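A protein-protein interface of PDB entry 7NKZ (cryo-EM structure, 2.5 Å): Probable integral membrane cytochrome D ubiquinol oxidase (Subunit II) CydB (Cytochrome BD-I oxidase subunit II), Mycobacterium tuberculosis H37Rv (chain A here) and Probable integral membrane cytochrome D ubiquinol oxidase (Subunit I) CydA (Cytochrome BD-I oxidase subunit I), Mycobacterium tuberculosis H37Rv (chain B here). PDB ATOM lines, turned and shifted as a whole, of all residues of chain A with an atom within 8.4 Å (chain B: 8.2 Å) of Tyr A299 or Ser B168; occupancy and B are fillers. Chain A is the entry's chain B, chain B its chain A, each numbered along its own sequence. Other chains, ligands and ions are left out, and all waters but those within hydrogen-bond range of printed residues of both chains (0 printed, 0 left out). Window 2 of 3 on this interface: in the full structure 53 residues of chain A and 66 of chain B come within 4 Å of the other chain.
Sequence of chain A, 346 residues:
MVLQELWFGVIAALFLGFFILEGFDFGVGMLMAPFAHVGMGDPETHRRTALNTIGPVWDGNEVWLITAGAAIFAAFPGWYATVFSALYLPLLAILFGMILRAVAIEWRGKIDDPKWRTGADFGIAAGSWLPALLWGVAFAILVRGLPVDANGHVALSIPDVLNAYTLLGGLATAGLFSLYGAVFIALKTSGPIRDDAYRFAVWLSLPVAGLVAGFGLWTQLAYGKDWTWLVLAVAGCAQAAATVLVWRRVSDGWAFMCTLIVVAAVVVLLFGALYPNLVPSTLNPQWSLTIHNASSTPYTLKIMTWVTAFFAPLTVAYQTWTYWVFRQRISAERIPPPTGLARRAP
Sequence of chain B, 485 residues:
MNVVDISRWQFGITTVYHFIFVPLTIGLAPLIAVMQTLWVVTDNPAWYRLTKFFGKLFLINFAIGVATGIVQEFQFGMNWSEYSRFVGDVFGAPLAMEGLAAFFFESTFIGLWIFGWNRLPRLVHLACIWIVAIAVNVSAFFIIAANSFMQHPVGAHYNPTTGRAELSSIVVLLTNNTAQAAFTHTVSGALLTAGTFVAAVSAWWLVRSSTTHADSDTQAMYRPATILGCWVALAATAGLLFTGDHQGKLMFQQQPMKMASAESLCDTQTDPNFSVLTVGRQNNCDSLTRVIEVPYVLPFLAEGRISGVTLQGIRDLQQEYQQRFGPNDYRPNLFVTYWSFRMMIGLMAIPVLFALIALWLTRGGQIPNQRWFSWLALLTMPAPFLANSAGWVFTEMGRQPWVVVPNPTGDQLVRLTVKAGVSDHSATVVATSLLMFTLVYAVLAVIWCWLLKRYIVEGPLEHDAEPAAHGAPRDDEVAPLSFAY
N of Thr A297 sits at hydrogen-bond distance from OD2 of Asp B89 (2.9 Å).
The side-chain hydroxyl of Tyr A299 is in hydrogen-bond range of the backbone NH of Ile B170 (3.0 Å).
OG1 of Thr A300 is in hydrogen-bond range of O of Asp B89, at 3.4 Å.
Of chain B, only Leu B167, Ser B168, Ser B169 and Ile B170 come within 4 Å of Tyr A299.
Ser B168 touches just one residue of chain A: Tyr A299 (3.3 Å).
Of chain A, only Tyr A299 (3.9 Å) and Thr A300 (3.7 Å) come within 4 Å of Leu B167.
Of chain A, only Tyr A299 (3.3 Å) comes within 4 Å of Ser B169.
Of the printed residues of chain B, Thr A297 touches Asp B89 (2.9 Å) and Glu B166 (3.5 Å).
Printed residues of chain B within 4 Å of Ile A303: Ile B170 (3.7 Å).
Val B172 touches none of the printed residues of chain A.
Asn B159 touches none of the printed residues of chain A.
The nearest residue of chain A that does not touch Ser B168 is Thr A300 (6.2 Å).
Hydrophobic or aromatic side chains of chain A within 4 Å of the printed part of chain B: Tyr A299 and Ile A303.
Among the printed residues, no Asp or Glu carboxylate lies within 4 Å of a Lys or Arg side-chain nitrogen of the other chain.
OG1 of Thr A297 is in hydrogen-bond range of OG1 of Thr A300 (3.1 Å).
OD1 of Asp B89 sits at hydrogen-bond distance from N of Leu B167, at 3.4 Å.
The backbone carbonyl oxygen (O) of Gly B155 is in hydrogen-bond range of the backbone NH (N) of Ser B168 (2.8 Å).
The backbone carbonyl oxygen (O) of Gly B155 sits at hydrogen-bond distance from the backbone NH (N) of Ser B169 (3.4 Å).
ND1 of His B157 lies within hydrogen-bond range of OG of Ser B168 (2.5 Å).
ND2 of Asn B159 lies close to OE2 of Glu B166.
Among the printed residues, pairs that only touch across the chains: Tyr A299 with Ser B169, Tyr A299 with Ser B168, Ser A296 with Asp B89, Thr A297 with Glu B166, Thr A300 with Leu B167, Ile A303 with Ile B170 and Tyr A299 with Leu B167.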
ATOM      1  N   MET A   1       4.454 -22.592   1.204  1.00  0.00           N
ATOM      2  CA  MET A   1       5.450 -23.034   0.236  1.00  0.00           C
ATOM      3  C   MET A   1       6.064 -21.865  -0.528  1.00  0.00           C
ATOM      4  O   MET A   1       5.841 -20.710  -0.187  1.00  0.00           O
ATOM      5  CB  MET A   1       4.857 -24.072  -0.719  1.00  0.00           C
ATOM      6  CG  MET A   1       3.471 -23.733  -1.242  1.00  0.00           C
ATOM      7  SD  MET A   1       3.503 -22.625  -2.661  1.00  0.00           S
ATOM      8  CE  MET A   1       1.766 -22.563  -3.090  1.00  0.00           C
ATOM      9  N   LEU A   3       5.691 -20.517  -3.844  1.00  0.00           N
ATOM     10  CA  LEU A   3       4.828 -19.535  -4.492  1.00  0.00           C
ATOM     11  C   LEU A   3       4.091 -18.674  -3.475  1.00  0.00           C
ATOM     12  O   LEU A   3       3.864 -17.484  -3.723  1.00  0.00           O
ATOM     13  CB  LEU A   3       3.831 -20.237  -5.413  1.00  0.00           C
ATOM     14  CG  LEU A   3       4.389 -20.791  -6.725  1.00  0.00           C
ATOM     15  CD1 LEU A   3       3.289 -21.451  -7.539  1.00  0.00           C
ATOM     16  CD2 LEU A   3       5.066 -19.689  -7.525  1.00  0.00           C
ATOM     17  N   TRP A   7       4.660 -14.631  -3.659  1.00  0.00           N
ATOM     18  CA  TRP A   7       3.585 -13.682  -3.919  1.00  0.00           C
ATOM     19  C   TRP A   7       3.392 -12.689  -2.782  1.00  0.00           C
ATOM     20  O   TRP A   7       2.778 -11.639  -2.995  1.00  0.00           O
ATOM     21  CB  TRP A   7       2.277 -14.424  -4.196  1.00  0.00           C
ATOM     22  CG  TRP A   7       1.928 -14.454  -5.648  1.00  0.00           C
ATOM     23  CD1 TRP A   7       2.107 -15.490  -6.516  1.00  0.00           C
ATOM     24  CD2 TRP A   7       1.353 -13.386  -6.411  1.00  0.00           C
ATOM     25  NE1 TRP A   7       1.672 -15.138  -7.770  1.00  0.00           N
ATOM     26  CE2 TRP A   7       1.205 -13.850  -7.732  1.00  0.00           C
ATOM     27  CE3 TRP A   7       0.946 -12.084  -6.103  1.00  0.00           C
ATOM     28  CZ2 TRP A   7       0.667 -13.059  -8.745  1.00  0.00           C
ATOM     29  CZ3 TRP A   7       0.412 -11.300  -7.110  1.00  0.00           C
ATOM     30  CH2 TRP A   7       0.278 -11.790  -8.415  1.00  0.00           C
ATOM     31  N   SER A 296      -4.146 -18.925  -2.080  1.00  0.00           N
ATOM     32  CA  SER A 296      -4.812 -19.706  -3.108  1.00  0.00           C
ATOM     33  C   SER A 296      -4.041 -20.999  -3.366  1.00  0.00           C
ATOM     34  O   SER A 296      -3.011 -21.276  -2.745  1.00  0.00           O
ATOM     35  CB  SER A 296      -4.956 -18.887  -4.390  1.00  0.00           C
ATOM     36  OG  SER A 296      -5.783 -17.755  -4.185  1.00  0.00           O
ATOM     37  N   THR A 297      -4.548 -21.804  -4.295  1.00  0.00           N
ATOM     38  CA  THR A 297      -3.883 -23.039  -4.664  1.00  0.00           C
ATOM     39  C   THR A 297      -2.605 -22.747  -5.447  1.00  0.00           C
ATOM     40  O   THR A 297      -2.456 -21.672  -6.032  1.00  0.00           O
ATOM     41  CB  THR A 297      -4.815 -23.920  -5.492  1.00  0.00           C
ATOM     42  OG1 THR A 297      -5.298 -23.183  -6.623  1.00  0.00           O
ATOM     43  CG2 THR A 297      -5.982 -24.392  -4.651  1.00  0.00           C
ATOM     44  N   PRO A 298      -1.657 -23.689  -5.455  1.00  0.00           N
ATOM     45  CA  PRO A 298      -0.436 -23.480  -6.250  1.00  0.00           C
ATOM     46  C   PRO A 298      -0.706 -23.259  -7.726  1.00  0.00           C
ATOM     47  O   PRO A 298       0.034 -22.505  -8.370  1.00  0.00           O
ATOM     48  CB  PRO A 298       0.362 -24.769  -6.006  1.00  0.00           C
ATOM     49  CG  PRO A 298      -0.126 -25.268  -4.691  1.00  0.00           C
ATOM     50  CD  PRO A 298      -1.583 -24.916  -4.641  1.00  0.00           C
ATOM     51  N   TYR A 299      -1.738 -23.894  -8.287  1.00  0.00           N
ATOM     52  CA  TYR A 299      -2.055 -23.679  -9.697  1.00  0.00           C
ATOM     53  C   TYR A 299      -2.453 -22.233  -9.962  1.00  0.00           C
ATOM     54  O   TYR A 299      -2.013 -21.635 -10.951  1.00  0.00           O
ATOM     55  CB  TYR A 299      -3.166 -24.629 -10.142  1.00  0.00           C
ATOM     56  CG  TYR A 299      -3.606 -24.408 -11.572  1.00  0.00           C
ATOM     57  CD1 TYR A 299      -2.859 -24.903 -12.632  1.00  0.00           C
ATOM     58  CD2 TYR A 299      -4.765 -23.700 -11.864  1.00  0.00           C
ATOM     59  CE1 TYR A 299      -3.252 -24.702 -13.941  1.00  0.00           C
ATOM     60  CE2 TYR A 299      -5.168 -23.493 -13.170  1.00  0.00           C
ATOM     61  CZ  TYR A 299      -4.407 -23.997 -14.204  1.00  0.00           C
ATOM     62  OH  TYR A 299      -4.801 -23.795 -15.507  1.00  0.00           O
ATOM     63  N   THR A 300      -3.290 -21.656  -9.096  1.00  0.00           N
ATOM     64  CA  THR A 300      -3.668 -20.256  -9.258  1.00  0.00           C
ATOM     65  C   THR A 300      -2.463 -19.339  -9.093  1.00  0.00           C
ATOM     66  O   THR A 300      -2.294 -18.383  -9.860  1.00  0.00           O
ATOM     67  CB  THR A 300      -4.764 -19.887  -8.259  1.00  0.00           C
ATOM     68  OG1 THR A 300      -5.893 -20.751  -8.446  1.00  0.00           O
ATOM     69  CG2 THR A 300      -5.204 -18.444  -8.455  1.00  0.00           C
ATOM     70  N   LEU A 301      -1.634 -19.607  -8.093  1.00  0.00           N
ATOM     71  CA  LEU A 301      -0.454 -18.791  -7.860  1.00  0.00           C
ATOM     72  C   LEU A 301       0.551 -18.998  -8.976  1.00  0.00           C
ATOM     73  O   LEU A 301       1.328 -18.108  -9.293  1.00  0.00           O
ATOM     74  CB  LEU A 301       0.180 -19.132  -6.517  1.00  0.00           C
ATOM     75  CG  LEU A 301      -0.643 -18.770  -5.285  1.00  0.00           C
ATOM     76  CD1 LEU A 301       0.106 -19.138  -4.019  1.00  0.00           C
ATOM     77  CD2 LEU A 301      -1.005 -17.295  -5.291  1.00  0.00           C
ATOM     78  N   LYS A 302       0.531 -20.183  -9.570  1.00  0.00           N
ATOM     79  CA  LYS A 302       1.444 -20.505 -10.653  1.00  0.00           C
ATOM     80  C   LYS A 302       1.021 -19.783 -11.921  1.00  0.00           C
ATOM     81  O   LYS A 302       1.830 -19.157 -12.594  1.00  0.00           O
ATOM     82  CB  LYS A 302       1.483 -22.014 -10.876  1.00  0.00           C
ATOM     83  CG  LYS A 302       2.461 -22.460 -11.942  1.00  0.00           C
ATOM     84  CD  LYS A 302       1.748 -22.825 -13.228  1.00  0.00           C
ATOM     85  CE  LYS A 302       0.991 -24.130 -13.063  1.00  0.00           C
ATOM     86  NZ  LYS A 302       0.455 -24.626 -14.359  1.00  0.00           N
ATOM     87  N   ILE A 303      -0.261 -19.877 -12.236  1.00  0.00           N
ATOM     88  CA  ILE A 303      -0.834 -19.228 -13.413  1.00  0.00           C
ATOM     89  C   ILE A 303      -0.650 -17.719 -13.329  1.00  0.00           C
ATOM     90  O   ILE A 303      -0.275 -17.067 -14.311  1.00  0.00           O
ATOM     91  CB  ILE A 303      -2.316 -19.617 -13.569  1.00  0.00           C
ATOM     92  CG1 ILE A 303      -2.439 -20.979 -14.254  1.00  0.00           C
ATOM     93  CG2 ILE A 303      -3.077 -18.556 -14.351  1.00  0.00           C
ATOM     94  CD1 ILE A 303      -1.704 -21.066 -15.574  1.00  0.00           C
ATOM     95  N   MET A 304      -0.899 -17.143 -12.152  1.00  0.00           N
ATOM     96  CA  MET A 304      -0.680 -15.715 -11.961  1.00  0.00           C
ATOM     97  C   MET A 304       0.796 -15.344 -12.000  1.00  0.00           C
ATOM     98  O   MET A 304       1.123 -14.195 -12.310  1.00  0.00           O
ATOM     99  CB  MET A 304      -1.295 -15.265 -10.636  1.00  0.00           C
ATOM    100  CG  MET A 304      -2.807 -15.132 -10.665  1.00  0.00           C
ATOM    101  SD  MET A 304      -3.334 -13.709 -11.637  1.00  0.00           S
ATOM    102  CE  MET A 304      -2.527 -12.386 -10.741  1.00  0.00           C
ATOM    103  N   THR A 305       1.691 -16.286 -11.684  1.00  0.00           N
ATOM    104  CA  THR A 305       3.119 -15.986 -11.707  1.00  0.00           C
ATOM    105  C   THR A 305       3.604 -15.681 -13.120  1.00  0.00           C
ATOM    106  O   THR A 305       4.358 -14.724 -13.328  1.00  0.00           O
ATOM    107  CB  THR A 305       3.911 -17.150 -11.110  1.00  0.00           C
ATOM    108  OG1 THR A 305       3.463 -17.395  -9.770  1.00  0.00           O
ATOM    109  CG2 THR A 305       5.397 -16.831 -11.087  1.00  0.00           C
ATOM    110  N   TRP A 306       3.181 -16.480 -14.104  1.00  0.00           N
ATOM    111  CA  TRP A 306       3.594 -16.232 -15.484  1.00  0.00           C
ATOM    112  C   TRP A 306       3.059 -14.900 -15.994  1.00  0.00           C
ATOM    113  O   TRP A 306       3.772 -14.162 -16.682  1.00  0.00           O
ATOM    114  CB  TRP A 306       3.135 -17.375 -16.391  1.00  0.00           C
ATOM    115  CG  TRP A 306       3.793 -18.690 -16.100  1.00  0.00           C
ATOM    116  CD1 TRP A 306       3.473 -19.564 -15.105  1.00  0.00           C
ATOM    117  CD2 TRP A 306       4.883 -19.281 -16.818  1.00  0.00           C
ATOM    118  NE1 TRP A 306       4.296 -20.663 -15.156  1.00  0.00           N
ATOM    119  CE2 TRP A 306       5.171 -20.514 -16.200  1.00  0.00           C
ATOM    120  CE3 TRP A 306       5.642 -18.888 -17.924  1.00  0.00           C
ATOM    121  CZ2 TRP A 306       6.185 -21.356 -16.649  1.00  0.00           C
ATOM    122  CZ3 TRP A 306       6.651 -19.725 -18.369  1.00  0.00           C
ATOM    123  CH2 TRP A 306       6.912 -20.945 -17.732  1.00  0.00           C
ATOM    124  N   ASP B  89     -10.209 -17.852  -5.292  1.00  0.00           N
ATOM    125  CA  ASP B  89      -9.269 -18.649  -6.071  1.00  0.00           C
ATOM    126  C   ASP B  89      -9.544 -18.574  -7.568  1.00  0.00           C
ATOM    127  O   ASP B  89      -8.622 -18.777  -8.365  1.00  0.00           O
ATOM    128  CB  ASP B  89      -9.311 -20.106  -5.605  1.00  0.00           C
ATOM    129  CG  ASP B  89      -7.985 -20.814  -5.784  1.00  0.00           C
ATOM    130  OD1 ASP B  89      -7.573 -21.025  -6.942  1.00  0.00           O
ATOM    131  OD2 ASP B  89      -7.353 -21.161  -4.763  1.00  0.00           O
ATOM    132  N   VAL B  90     -10.781 -18.284  -7.967  1.00  0.00           N
ATOM    133  CA  VAL B  90     -11.162 -18.230  -9.369  1.00  0.00           C
ATOM    134  C   VAL B  90     -11.478 -16.808  -9.814  1.00  0.00           C
ATOM    135  O   VAL B  90     -10.970 -16.348 -10.839  1.00  0.00           O
ATOM    136  CB  VAL B  90     -12.359 -19.165  -9.646  1.00  0.00           C
ATOM    137  CG1 VAL B  90     -12.485 -19.440 -11.137  1.00  0.00           C
ATOM    138  CG2 VAL B  90     -12.226 -20.457  -8.858  1.00  0.00           C
ATOM    139  N   PHE B 149     -18.161 -16.092 -15.009  1.00  0.00           N
ATOM    140  CA  PHE B 149     -17.999 -17.209 -14.086  1.00  0.00           C
ATOM    141  C   PHE B 149     -19.174 -17.301 -13.123  1.00  0.00           C
ATOM    142  O   PHE B 149     -19.597 -18.406 -12.761  1.00  0.00           O
ATOM    143  CB  PHE B 149     -16.683 -17.074 -13.319  1.00  0.00           C
ATOM    144  CG  PHE B 149     -16.477 -18.137 -12.276  1.00  0.00           C
ATOM    145  CD1 PHE B 149     -16.055 -19.406 -12.633  1.00  0.00           C
ATOM    146  CD2 PHE B 149     -16.700 -17.862 -10.936  1.00  0.00           C
ATOM    147  CE1 PHE B 149     -15.867 -20.385 -11.674  1.00  0.00           C
ATOM    148  CE2 PHE B 149     -16.512 -18.835  -9.974  1.00  0.00           C
ATOM    149  CZ  PHE B 149     -16.096 -20.098 -10.343  1.00  0.00           C
ATOM    150  N   VAL B 154     -17.126 -22.409 -15.025  1.00  0.00           N
ATOM    151  CA  VAL B 154     -16.429 -23.485 -15.718  1.00  0.00           C
ATOM    152  C   VAL B 154     -14.991 -23.534 -15.223  1.00  0.00           C
ATOM    153  O   VAL B 154     -14.440 -22.534 -14.754  1.00  0.00           O
ATOM    154  CB  VAL B 154     -16.470 -23.308 -17.253  1.00  0.00           C
ATOM    155  CG1 VAL B 154     -17.881 -23.520 -17.777  1.00  0.00           C
ATOM    156  CG2 VAL B 154     -15.950 -21.932 -17.642  1.00  0.00           C
ATOM    157  N   GLY B 155     -14.384 -24.712 -15.334  1.00  0.00           N
ATOM    158  CA  GLY B 155     -13.010 -24.891 -14.907  1.00  0.00           C
ATOM    159  C   GLY B 155     -12.776 -24.669 -13.430  1.00  0.00           C
ATOM    160  O   GLY B 155     -11.740 -24.114 -13.051  1.00  0.00           O
ATOM    161  N   ALA B 156     -13.714 -25.085 -12.583  1.00  0.00           N
ATOM    162  CA  ALA B 156     -13.576 -24.910 -11.146  1.00  0.00           C
ATOM    163  C   ALA B 156     -14.202 -26.099 -10.432  1.00  0.00           C
ATOM    164  O   ALA B 156     -15.170 -26.693 -10.917  1.00  0.00           O
ATOM    165  CB  ALA B 156     -14.222 -23.604 -10.671  1.00  0.00           C
ATOM    166  N   HIS B 157     -13.640 -26.437  -9.278  1.00  0.00           N
ATOM    167  CA  HIS B 157     -14.129 -27.521  -8.441  1.00  0.00           C
ATOM    168  C   HIS B 157     -14.433 -26.991  -7.044  1.00  0.00           C
ATOM    169  O   HIS B 157     -13.858 -25.998  -6.591  1.00  0.00           O
ATOM    170  CB  HIS B 157     -13.116 -28.671  -8.371  1.00  0.00           C
ATOM    171  CG  HIS B 157     -11.758 -28.252  -7.900  1.00  0.00           C
ATOM    172  ND1 HIS B 157     -10.815 -27.701  -8.739  1.00  0.00           N
ATOM    173  CD2 HIS B 157     -11.183 -28.307  -6.675  1.00  0.00           C
ATOM    174  CE1 HIS B 157      -9.720 -27.433  -8.053  1.00  0.00           C
ATOM    175  NE2 HIS B 157      -9.917 -27.791  -6.797  1.00  0.00           N
ATOM    176  N   TYR B 158     -15.357 -27.669  -6.362  1.00  0.00           N
ATOM    177  CA  TYR B 158     -15.786 -27.210  -5.046  1.00  0.00           C
ATOM    178  C   TYR B 158     -14.713 -27.424  -3.986  1.00  0.00           C
ATOM    179  O   TYR B 158     -14.543 -26.578  -3.101  1.00  0.00           O
ATOM    180  CB  TYR B 158     -17.080 -27.911  -4.635  1.00  0.00           C
ATOM    181  CG  TYR B 158     -17.594 -27.476  -3.281  1.00  0.00           C
ATOM    182  CD1 TYR B 158     -18.101 -26.198  -3.088  1.00  0.00           C
ATOM    183  CD2 TYR B 158     -17.571 -28.342  -2.197  1.00  0.00           C
ATOM    184  CE1 TYR B 158     -18.569 -25.794  -1.852  1.00  0.00           C
ATOM    185  CE2 TYR B 158     -18.039 -27.948  -0.958  1.00  0.00           C
ATOM    186  CZ  TYR B 158     -18.536 -26.674  -0.791  1.00  0.00           C
ATOM    187  OH  TYR B 158     -19.003 -26.276   0.441  1.00  0.00           O
ATOM    188  N   ASN B 159     -13.980 -28.541  -4.061  1.00  0.00           N
ATOM    189  CA  ASN B 159     -12.961 -28.893  -3.076  1.00  0.00           C
ATOM    190  C   ASN B 159     -13.545 -28.854  -1.669  1.00  0.00           C
ATOM    191  O   ASN B 159     -13.273 -27.915  -0.910  1.00  0.00           O
ATOM    192  CB  ASN B 159     -11.755 -27.957  -3.180  1.00  0.00           C
ATOM    193  CG  ASN B 159     -10.574 -28.434  -2.356  1.00  0.00           C
ATOM    194  OD1 ASN B 159     -10.406 -28.039  -1.203  1.00  0.00           O
ATOM    195  ND2 ASN B 159      -9.749 -29.291  -2.946  1.00  0.00           N
ATOM    196  N   ALA B 165     -14.571 -22.143  -3.768  1.00  0.00           N
ATOM    197  CA  ALA B 165     -14.396 -22.684  -5.108  1.00  0.00           C
ATOM    198  C   ALA B 165     -12.963 -22.447  -5.565  1.00  0.00           C
ATOM    199  O   ALA B 165     -12.416 -21.357  -5.368  1.00  0.00           O
ATOM    200  CB  ALA B 165     -15.380 -22.044  -6.086  1.00  0.00           C
ATOM    201  N   GLU B 166     -12.359 -23.463  -6.172  1.00  0.00           N
ATOM    202  CA  GLU B 166     -10.955 -23.425  -6.549  1.00  0.00           C
ATOM    203  C   GLU B 166     -10.806 -23.572  -8.057  1.00  0.00           C
ATOM    204  O   GLU B 166     -11.501 -24.375  -8.686  1.00  0.00           O
ATOM    205  CB  GLU B 166     -10.170 -24.529  -5.837  1.00  0.00           C
ATOM    206  CG  GLU B 166      -9.452 -24.050  -4.593  1.00  0.00           C
ATOM    207  CD  GLU B 166      -9.275 -25.148  -3.565  1.00  0.00           C
ATOM    208  OE1 GLU B 166      -9.333 -24.847  -2.354  1.00  0.00           O
ATOM    209  OE2 GLU B 166      -9.065 -26.311  -3.968  1.00  0.00           O
ATOM    210  N   LEU B 167      -9.892 -22.791  -8.629  1.00  0.00           N
ATOM    211  CA  LEU B 167      -9.676 -22.789 -10.069  1.00  0.00           C
ATOM    212  C   LEU B 167      -8.980 -24.072 -10.506  1.00  0.00           C
ATOM    213  O   LEU B 167      -8.021 -24.518  -9.868  1.00  0.00           O
ATOM    214  CB  LEU B 167      -8.850 -21.571 -10.481  1.00  0.00           C
ATOM    215  CG  LEU B 167      -8.502 -21.441 -11.965  1.00  0.00           C
ATOM    216  CD1 LEU B 167      -9.764 -21.374 -12.810  1.00  0.00           C
ATOM    217  CD2 LEU B 167      -7.626 -20.221 -12.205  1.00  0.00           C
ATOM    218  N   SER B 168      -9.466 -24.663 -11.597  1.00  0.00           N
ATOM    219  CA  SER B 168      -8.879 -25.868 -12.169  1.00  0.00           C
ATOM    220  C   SER B 168      -8.121 -25.600 -13.461  1.00  0.00           C
ATOM    221  O   SER B 168      -7.034 -26.150 -13.661  1.00  0.00           O
ATOM    222  CB  SER B 168      -9.965 -26.916 -12.426  1.00  0.00           C
ATOM    223  OG  SER B 168     -10.621 -27.277 -11.223  1.00  0.00           O
ATOM    224  N   SER B 169      -8.670 -24.767 -14.344  1.00  0.00           N
ATOM    225  CA  SER B 169      -8.011 -24.435 -15.601  1.00  0.00           C
ATOM    226  C   SER B 169      -8.304 -22.982 -15.943  1.00  0.00           C
ATOM    227  O   SER B 169      -9.468 -22.575 -15.980  1.00  0.00           O
ATOM    228  CB  SER B 169      -8.480 -25.354 -16.733  1.00  0.00           C
ATOM    229  OG  SER B 169      -7.851 -25.018 -17.957  1.00  0.00           O
ATOM    230  N   ILE B 170      -7.247 -22.209 -16.191  1.00  0.00           N
ATOM    231  CA  ILE B 170      -7.427 -20.803 -16.538  1.00  0.00           C
ATOM    232  C   ILE B 170      -7.908 -20.652 -17.979  1.00  0.00           C
ATOM    233  O   ILE B 170      -8.613 -19.689 -18.302  1.00  0.00           O
ATOM    234  CB  ILE B 170      -6.125 -20.022 -16.287  1.00  0.00           C
ATOM    235  CG1 ILE B 170      -6.349 -18.518 -16.465  1.00  0.00           C
ATOM    236  CG2 ILE B 170      -5.009 -20.516 -17.198  1.00  0.00           C
ATOM    237  CD1 ILE B 170      -7.374 -17.937 -15.515  1.00  0.00           C
ATOM    238  N   VAL B 171      -7.547 -21.589 -18.859  1.00  0.00           N
ATOM    239  CA  VAL B 171      -7.980 -21.511 -20.251  1.00  0.00           C
ATOM    240  C   VAL B 171      -9.494 -21.655 -20.350  1.00  0.00           C
ATOM    241  O   VAL B 171     -10.156 -20.908 -21.081  1.00  0.00           O
ATOM    242  CB  VAL B 171      -7.247 -22.571 -21.094  1.00  0.00           C
ATOM    243  CG1 VAL B 171      -8.029 -22.886 -22.362  1.00  0.00           C
ATOM    244  CG2 VAL B 171      -5.841 -22.100 -21.430  1.00  0.00           C
ATOM    245  N   VAL B 172     -10.067 -22.607 -19.611  1.00  0.00           N
ATOM    246  CA  VAL B 172     -11.512 -22.812 -19.646  1.00  0.00           C
ATOM    247  C   VAL B 172     -12.247 -21.597 -19.095  1.00  0.00           C
ATOM    248  O   VAL B 172     -13.293 -21.204 -19.624  1.00  0.00           O
ATOM    249  CB  VAL B 172     -11.886 -24.094 -18.879  1.00  0.00           C
ATOM    250  CG1 VAL B 172     -13.370 -24.385 -19.021  1.00  0.00           C
ATOM    251  CG2 VAL B 172     -11.059 -25.267 -19.378  1.00  0.00           C
ATOM    252  N   LEU B 173     -11.723 -20.987 -18.029  1.00  0.00           N
ATOM    253  CA  LEU B 173     -12.363 -19.804 -17.461  1.00  0.00           C
ATOM    254  C   LEU B 173     -12.372 -18.645 -18.450  1.00  0.00           C
ATOM    255  O   LEU B 173     -13.383 -17.946 -18.587  1.00  0.00           O
ATOM    256  CB  LEU B 173     -11.658 -19.400 -16.167  1.00  0.00           C
ATOM    257  CG  LEU B 173     -12.163 -18.130 -15.479  1.00  0.00           C
ATOM    258  CD1 LEU B 173     -13.612 -18.290 -15.051  1.00  0.00           C
ATOM    259  CD2 LEU B 173     -11.285 -17.776 -14.289  1.00  0.00           C
ATOM    260  N   ASP B 411     -20.071 -28.288 -12.027  1.00  0.00           N
ATOM    261  CA  ASP B 411     -20.110 -28.757 -10.648  1.00  0.00           C
ATOM    262  C   ASP B 411     -21.324 -28.159  -9.947  1.00  0.00           C
ATOM    263  O   ASP B 411     -21.488 -26.934  -9.908  1.00  0.00           O
ATOM    264  CB  ASP B 411     -18.816 -28.376  -9.929  1.00  0.00           C
ATOM    265  CG  ASP B 411     -18.703 -28.981  -8.535  1.00  0.00           C
ATOM    266  OD1 ASP B 411     -19.737 -29.274  -7.898  1.00  0.00           O
ATOM    267  OD2 ASP B 411     -17.559 -29.165  -8.070  1.00  0.00           O
ATOM    268  N   VAL B 414     -20.505 -25.925  -6.745  1.00  0.00           N
ATOM    269  CA  VAL B 414     -19.933 -24.600  -6.949  1.00  0.00           C
ATOM    270  C   VAL B 414     -21.073 -23.616  -7.175  1.00  0.00           C
ATOM    271  O   VAL B 414     -21.518 -23.407  -8.310  1.00  0.00           O
ATOM    272  CB  VAL B 414     -18.935 -24.588  -8.123  1.00  0.00           C
ATOM    273  CG1 VAL B 414     -18.399 -23.180  -8.358  1.00  0.00           C
ATOM    274  CG2 VAL B 414     -17.794 -25.554  -7.856  1.00  0.00           C
